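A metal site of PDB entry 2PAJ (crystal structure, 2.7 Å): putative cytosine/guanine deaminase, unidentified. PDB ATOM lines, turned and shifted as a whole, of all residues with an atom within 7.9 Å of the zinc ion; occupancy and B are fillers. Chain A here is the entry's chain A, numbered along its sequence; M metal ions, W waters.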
ATOM      1  N   HIS A  76     -12.353  28.374 -25.323  1.00  0.00           N
ATOM      2  CA  HIS A  76     -11.138  28.823 -24.653  1.00  0.00           C
ATOM      3  C   HIS A  76      -9.933  27.988 -25.068  1.00  0.00           C
ATOM      4  O   HIS A  76     -10.014  26.765 -25.124  1.00  0.00           O
ATOM      5  CB  HIS A  76     -11.304  28.798 -23.136  1.00  0.00           C
ATOM      6  CG  HIS A  76     -10.146  29.379 -22.393  1.00  0.00           C
ATOM      7  ND1 HIS A  76      -9.759  30.698 -22.533  1.00  0.00           N
ATOM      8  CD2 HIS A  76      -9.243  28.809 -21.563  1.00  0.00           C
ATOM      9  CE1 HIS A  76      -8.670  30.913 -21.817  1.00  0.00           C
ATOM     10  NE2 HIS A  76      -8.336  29.778 -21.216  1.00  0.00           N
ATOM     11  N   HIS A  77      -8.812  28.649 -25.354  1.00  0.00           N
ATOM     12  CA  HIS A  77      -7.601  27.982 -25.836  1.00  0.00           C
ATOM     13  C   HIS A  77      -6.374  28.902 -25.756  1.00  0.00           C
ATOM     14  O   HIS A  77      -6.494  30.080 -25.466  1.00  0.00           O
ATOM     15  CB  HIS A  77      -7.807  27.584 -27.293  1.00  0.00           C
ATOM     16  CG  HIS A  77      -7.029  26.375 -27.718  1.00  0.00           C
ATOM     17  ND1 HIS A  77      -5.799  26.047 -27.187  1.00  0.00           N
ATOM     18  CD2 HIS A  77      -7.292  25.431 -28.661  1.00  0.00           C
ATOM     19  CE1 HIS A  77      -5.330  24.960 -27.785  1.00  0.00           C
ATOM     20  NE2 HIS A  77      -6.221  24.569 -28.685  1.00  0.00           N
ATOM     21  N   HIS A  78      -5.201  28.331 -26.020  1.00  0.00           N
ATOM     22  CA  HIS A  78      -3.933  29.059 -26.049  1.00  0.00           C
ATOM     23  C   HIS A  78      -3.060  28.329 -27.081  1.00  0.00           C
ATOM     24  O   HIS A  78      -2.049  27.742 -26.723  1.00  0.00           O
ATOM     25  CB  HIS A  78      -3.238  29.038 -24.682  1.00  0.00           C
ATOM     26  CG  HIS A  78      -4.039  29.641 -23.576  1.00  0.00           C
ATOM     27  ND1 HIS A  78      -4.562  30.914 -23.647  1.00  0.00           N
ATOM     28  CD2 HIS A  78      -4.417  29.143 -22.375  1.00  0.00           C
ATOM     29  CE1 HIS A  78      -5.223  31.173 -22.527  1.00  0.00           C
ATOM     30  NE2 HIS A  78      -5.149  30.111 -21.746  1.00  0.00           N
ATOM     31  N   GLN A  81       0.761  27.399 -27.238  1.00  0.00           N
ATOM     32  CA  GLN A  81       1.189  26.352 -26.311  1.00  0.00           C
ATOM     33  C   GLN A  81       1.231  24.962 -26.947  1.00  0.00           C
ATOM     34  O   GLN A  81       1.740  24.026 -26.349  1.00  0.00           O
ATOM     35  CB  GLN A  81       0.262  26.347 -25.102  1.00  0.00           C
ATOM     36  CG  GLN A  81       0.682  27.349 -24.063  1.00  0.00           C
ATOM     37  CD  GLN A  81      -0.436  27.733 -23.130  1.00  0.00           C
ATOM     38  OE1 GLN A  81      -1.173  26.878 -22.624  1.00  0.00           O
ATOM     39  NE2 GLN A  81      -0.576  29.026 -22.881  1.00  0.00           N
ATOM     40  N   HIS A 137      -7.516  32.168 -27.001  1.00  0.00           N
ATOM     41  CA  HIS A 137      -7.214  33.277 -26.097  1.00  0.00           C
ATOM     42  C   HIS A 137      -5.745  33.563 -26.360  1.00  0.00           C
ATOM     43  O   HIS A 137      -4.866  33.137 -25.613  1.00  0.00           O
ATOM     44  CB  HIS A 137      -7.438  32.866 -24.631  1.00  0.00           C
ATOM     45  CG  HIS A 137      -7.405  34.022 -23.676  1.00  0.00           C
ATOM     46  ND1 HIS A 137      -7.500  33.856 -22.309  1.00  0.00           N
ATOM     47  CD2 HIS A 137      -7.286  35.350 -23.881  1.00  0.00           C
ATOM     48  CE1 HIS A 137      -7.456  35.033 -21.713  1.00  0.00           C
ATOM     49  NE2 HIS A 137      -7.322  35.960 -22.650  1.00  0.00           N
ATOM     50  N   TYR A 139      -2.412  35.634 -26.545  1.00  0.00           N
ATOM     51  CA  TYR A 139      -1.834  36.723 -25.790  1.00  0.00           C
ATOM     52  C   TYR A 139      -0.372  36.977 -26.106  1.00  0.00           C
ATOM     53  O   TYR A 139       0.349  37.633 -25.336  1.00  0.00           O
ATOM     54  CB  TYR A 139      -2.062  36.563 -24.290  1.00  0.00           C
ATOM     55  CG  TYR A 139      -1.527  35.312 -23.653  1.00  0.00           C
ATOM     56  CD1 TYR A 139      -0.161  35.128 -23.487  1.00  0.00           C
ATOM     57  CD2 TYR A 139      -2.397  34.372 -23.132  1.00  0.00           C
ATOM     58  CE1 TYR A 139       0.335  34.035 -22.818  1.00  0.00           C
ATOM     59  CE2 TYR A 139      -1.935  33.263 -22.458  1.00  0.00           C
ATOM     60  CZ  TYR A 139      -0.566  33.102 -22.300  1.00  0.00           C
ATOM     61  OH  TYR A 139      -0.092  32.012 -21.632  1.00  0.00           O
ATOM     62  N   THR A 220      -5.790  38.929 -20.790  1.00  0.00           N
ATOM     63  CA  THR A 220      -5.475  37.657 -20.138  1.00  0.00           C
ATOM     64  C   THR A 220      -6.132  37.369 -18.776  1.00  0.00           C
ATOM     65  O   THR A 220      -7.107  36.615 -18.708  1.00  0.00           O
ATOM     66  CB  THR A 220      -3.966  37.493 -20.006  1.00  0.00           C
ATOM     67  OG1 THR A 220      -3.340  38.034 -21.176  1.00  0.00           O
ATOM     68  CG2 THR A 220      -3.607  36.004 -19.889  1.00  0.00           C
ATOM     69  N   HIS A 246     -13.920  38.574 -22.664  1.00  0.00           N
ATOM     70  CA  HIS A 246     -13.514  37.296 -22.099  1.00  0.00           C
ATOM     71  C   HIS A 246     -12.191  37.405 -21.359  1.00  0.00           C
ATOM     72  O   HIS A 246     -11.301  38.132 -21.785  1.00  0.00           O
ATOM     73  CB  HIS A 246     -13.409  36.266 -23.206  1.00  0.00           C
ATOM     74  CG  HIS A 246     -12.794  34.968 -22.769  1.00  0.00           C
ATOM     75  ND1 HIS A 246     -11.565  34.550 -23.216  1.00  0.00           N
ATOM     76  CD2 HIS A 246     -13.241  34.011 -21.925  1.00  0.00           C
ATOM     77  CE1 HIS A 246     -11.274  33.391 -22.658  1.00  0.00           C
ATOM     78  NE2 HIS A 246     -12.273  33.035 -21.869  1.00  0.00           N
ATOM     79  N   SER A 247     -12.051  36.673 -20.262  1.00  0.00           N
ATOM     80  CA  SER A 247     -10.814  36.686 -19.490  1.00  0.00           C
ATOM     81  C   SER A 247     -10.688  35.512 -18.507  1.00  0.00           C
ATOM     82  O   SER A 247     -11.661  34.812 -18.225  1.00  0.00           O
ATOM     83  CB  SER A 247     -10.683  38.013 -18.712  1.00  0.00           C
ATOM     84  OG  SER A 247      -9.450  38.113 -18.025  1.00  0.00           O
ATOM     85  N   HIS A 248      -9.458  35.307 -18.026  1.00  0.00           N
ATOM     86  CA  HIS A 248      -9.136  34.290 -17.034  1.00  0.00           C
ATOM     87  C   HIS A 248      -9.529  34.915 -15.696  1.00  0.00           C
ATOM     88  O   HIS A 248      -9.029  35.985 -15.336  1.00  0.00           O
ATOM     89  CB  HIS A 248      -7.622  34.038 -17.027  1.00  0.00           C
ATOM     90  CG  HIS A 248      -7.164  32.950 -17.959  1.00  0.00           C
ATOM     91  ND1 HIS A 248      -5.978  33.027 -18.649  1.00  0.00           N
ATOM     92  CD2 HIS A 248      -7.681  31.725 -18.236  1.00  0.00           C
ATOM     93  CE1 HIS A 248      -5.779  31.901 -19.307  1.00  0.00           C
ATOM     94  NE2 HIS A 248      -6.795  31.100 -19.077  1.00  0.00           N
ATOM     95  N   ALA A 284     -12.951  32.127 -18.086  1.00  0.00           N
ATOM     96  CA  ALA A 284     -12.261  30.842 -18.090  1.00  0.00           C
ATOM     97  C   ALA A 284     -11.578  30.694 -16.737  1.00  0.00           C
ATOM     98  O   ALA A 284     -11.370  31.664 -16.012  1.00  0.00           O
ATOM     99  CB  ALA A 284     -11.229  30.804 -19.199  1.00  0.00           C
ATOM    100  N   HIS A 285     -11.228  29.453 -16.399  1.00  0.00           N
ATOM    101  CA  HIS A 285     -10.548  29.118 -15.158  1.00  0.00           C
ATOM    102  C   HIS A 285     -11.148  29.731 -13.915  1.00  0.00           C
ATOM    103  O   HIS A 285     -10.436  30.268 -13.068  1.00  0.00           O
ATOM    104  CB  HIS A 285      -9.060  29.516 -15.267  1.00  0.00           C
ATOM    105  CG  HIS A 285      -8.335  28.808 -16.376  1.00  0.00           C
ATOM    106  ND1 HIS A 285      -8.989  28.138 -17.392  1.00  0.00           N
ATOM    107  CD2 HIS A 285      -7.009  28.692 -16.651  1.00  0.00           C
ATOM    108  CE1 HIS A 285      -8.109  27.634 -18.239  1.00  0.00           C
ATOM    109  NE2 HIS A 285      -6.904  27.965 -17.817  1.00  0.00           N
ATOM    110  N   CYS A 307     -13.037  24.096 -18.333  1.00  0.00           N
ATOM    111  CA  CYS A 307     -11.889  23.333 -18.813  1.00  0.00           C
ATOM    112  C   CYS A 307     -11.389  22.343 -17.753  1.00  0.00           C
ATOM    113  O   CYS A 307     -10.431  22.622 -17.045  1.00  0.00           O
ATOM    114  CB  CYS A 307     -10.740  24.287 -19.207  1.00  0.00           C
ATOM    115  SG  CYS A 307     -11.160  25.544 -20.452  1.00  0.00           S
ATOM    116  N   SER A 310      -7.553  20.767 -17.882  1.00  0.00           N
ATOM    117  CA  SER A 310      -6.599  21.816 -17.548  1.00  0.00           C
ATOM    118  C   SER A 310      -6.769  22.205 -16.087  1.00  0.00           C
ATOM    119  O   SER A 310      -5.792  22.292 -15.346  1.00  0.00           O
ATOM    120  CB  SER A 310      -6.850  23.020 -18.450  1.00  0.00           C
ATOM    121  OG  SER A 310      -5.751  23.918 -18.405  1.00  0.00           O
ATOM    122  N   ASN A 311      -8.012  22.436 -15.666  1.00  0.00           N
ATOM    123  CA  ASN A 311      -8.298  22.817 -14.282  1.00  0.00           C
ATOM    124  C   ASN A 311      -7.826  21.781 -13.273  1.00  0.00           C
ATOM    125  O   ASN A 311      -7.777  22.062 -12.079  1.00  0.00           O
ATOM    126  CB  ASN A 311      -9.805  23.091 -14.100  1.00  0.00           C
ATOM    127  CG  ASN A 311     -10.266  24.337 -14.839  1.00  0.00           C
ATOM    128  OD1 ASN A 311      -9.469  25.248 -15.127  1.00  0.00           O
ATOM    129  ND2 ASN A 311     -11.560  24.394 -15.141  1.00  0.00           N
ATOM    130  N   VAL A 335     -10.704  23.829 -23.944  1.00  0.00           N
ATOM    131  CA  VAL A 335      -9.519  23.044 -23.619  1.00  0.00           C
ATOM    132  C   VAL A 335      -8.455  24.105 -23.842  1.00  0.00           C
ATOM    133  O   VAL A 335      -8.329  24.585 -24.972  1.00  0.00           O
ATOM    134  CB  VAL A 335      -9.339  21.876 -24.641  1.00  0.00           C
ATOM    135  CG1 VAL A 335     -10.603  21.695 -25.414  1.00  0.00           C
ATOM    136  CG2 VAL A 335      -8.175  22.151 -25.620  1.00  0.00           C
ATOM    137  N   ASP A 336      -7.704  24.517 -22.835  1.00  0.00           N
ATOM    138  CA  ASP A 336      -6.743  25.571 -23.139  1.00  0.00           C
ATOM    139  C   ASP A 336      -5.267  25.235 -23.146  1.00  0.00           C
ATOM    140  O   ASP A 336      -4.761  24.608 -22.232  1.00  0.00           O
ATOM    141  CB  ASP A 336      -6.974  26.805 -22.261  1.00  0.00           C
ATOM    142  CG  ASP A 336      -6.595  26.591 -20.799  1.00  0.00           C
ATOM    143  OD1 ASP A 336      -5.856  27.453 -20.259  1.00  0.00           O
ATOM    144  OD2 ASP A 336      -7.035  25.608 -20.183  1.00  0.00           O
ATOM    145  N   GLY A 337      -4.573  25.656 -24.191  1.00  0.00           N
ATOM    146  CA  GLY A 337      -3.132  25.408 -24.294  1.00  0.00           C
ATOM    147  C   GLY A 337      -2.563  24.081 -23.810  1.00  0.00           C
ATOM    148  O   GLY A 337      -2.673  23.732 -22.641  1.00  0.00           O
ATOM    149  N   SER A 340      -1.011  23.122 -20.390  1.00  0.00           N
ATOM    150  CA  SER A 340      -1.745  22.765 -19.192  1.00  0.00           C
ATOM    151  C   SER A 340      -2.664  21.577 -19.462  1.00  0.00           C
ATOM    152  O   SER A 340      -3.144  20.937 -18.546  1.00  0.00           O
ATOM    153  CB  SER A 340      -2.560  23.968 -18.742  1.00  0.00           C
ATOM    154  OG  SER A 340      -3.300  23.663 -17.581  1.00  0.00           O
HETATM  155 ZN    ZN M   1      -6.316  29.441 -20.196  1.00  0.00          ZN
HETATM  156  O   HOH W   1      -4.283  28.935 -18.561  1.00  0.00           O
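Merely in contact with the zinc ion: His 285.
Along chain A the residues within 4 Å of the zinc ion span positions 76 to 336.
The nearest printed residue that does not touch the zinc ion is His 137 (5.0 Å).
The zinc ion is bound by OD1 of Asp 336 (2.0 Å), NE2 of His 78 (2.1 Å), NE2 of His 248 (2.1 Å) and NE2 of His 76 (2.3 Å).
Slightly farther from the zinc ion lies water W1 (2.7 Å).
OD2 of Asp 336 sits close to NE2 of His 285 (3.3 Å).
The side-chain carboxylate (OD2) of Asp 336 sits at hydrogen-bond distance from the side-chain hydroxyl (OG) of Ser 310, 2.8 Å away.
ND1 of His 78 sits at hydrogen-bond distance from O of His 137, at 3.0 Å.
A ring nitrogen (NE2) of His 248 lies close to a ring nitrogen (NE2) of His 285 (3.4 Å).
The backbone NH (N) of His 248 sits at hydrogen-bond distance from the backbone carbonyl oxygen (O) of Thr 220 (2.8 Å).
A ring nitrogen (ND1) of His 76 sits close to a ring nitrogen (NE2) of His 246.
N of Val 335 sits at hydrogen-bond distance from O of His 76.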
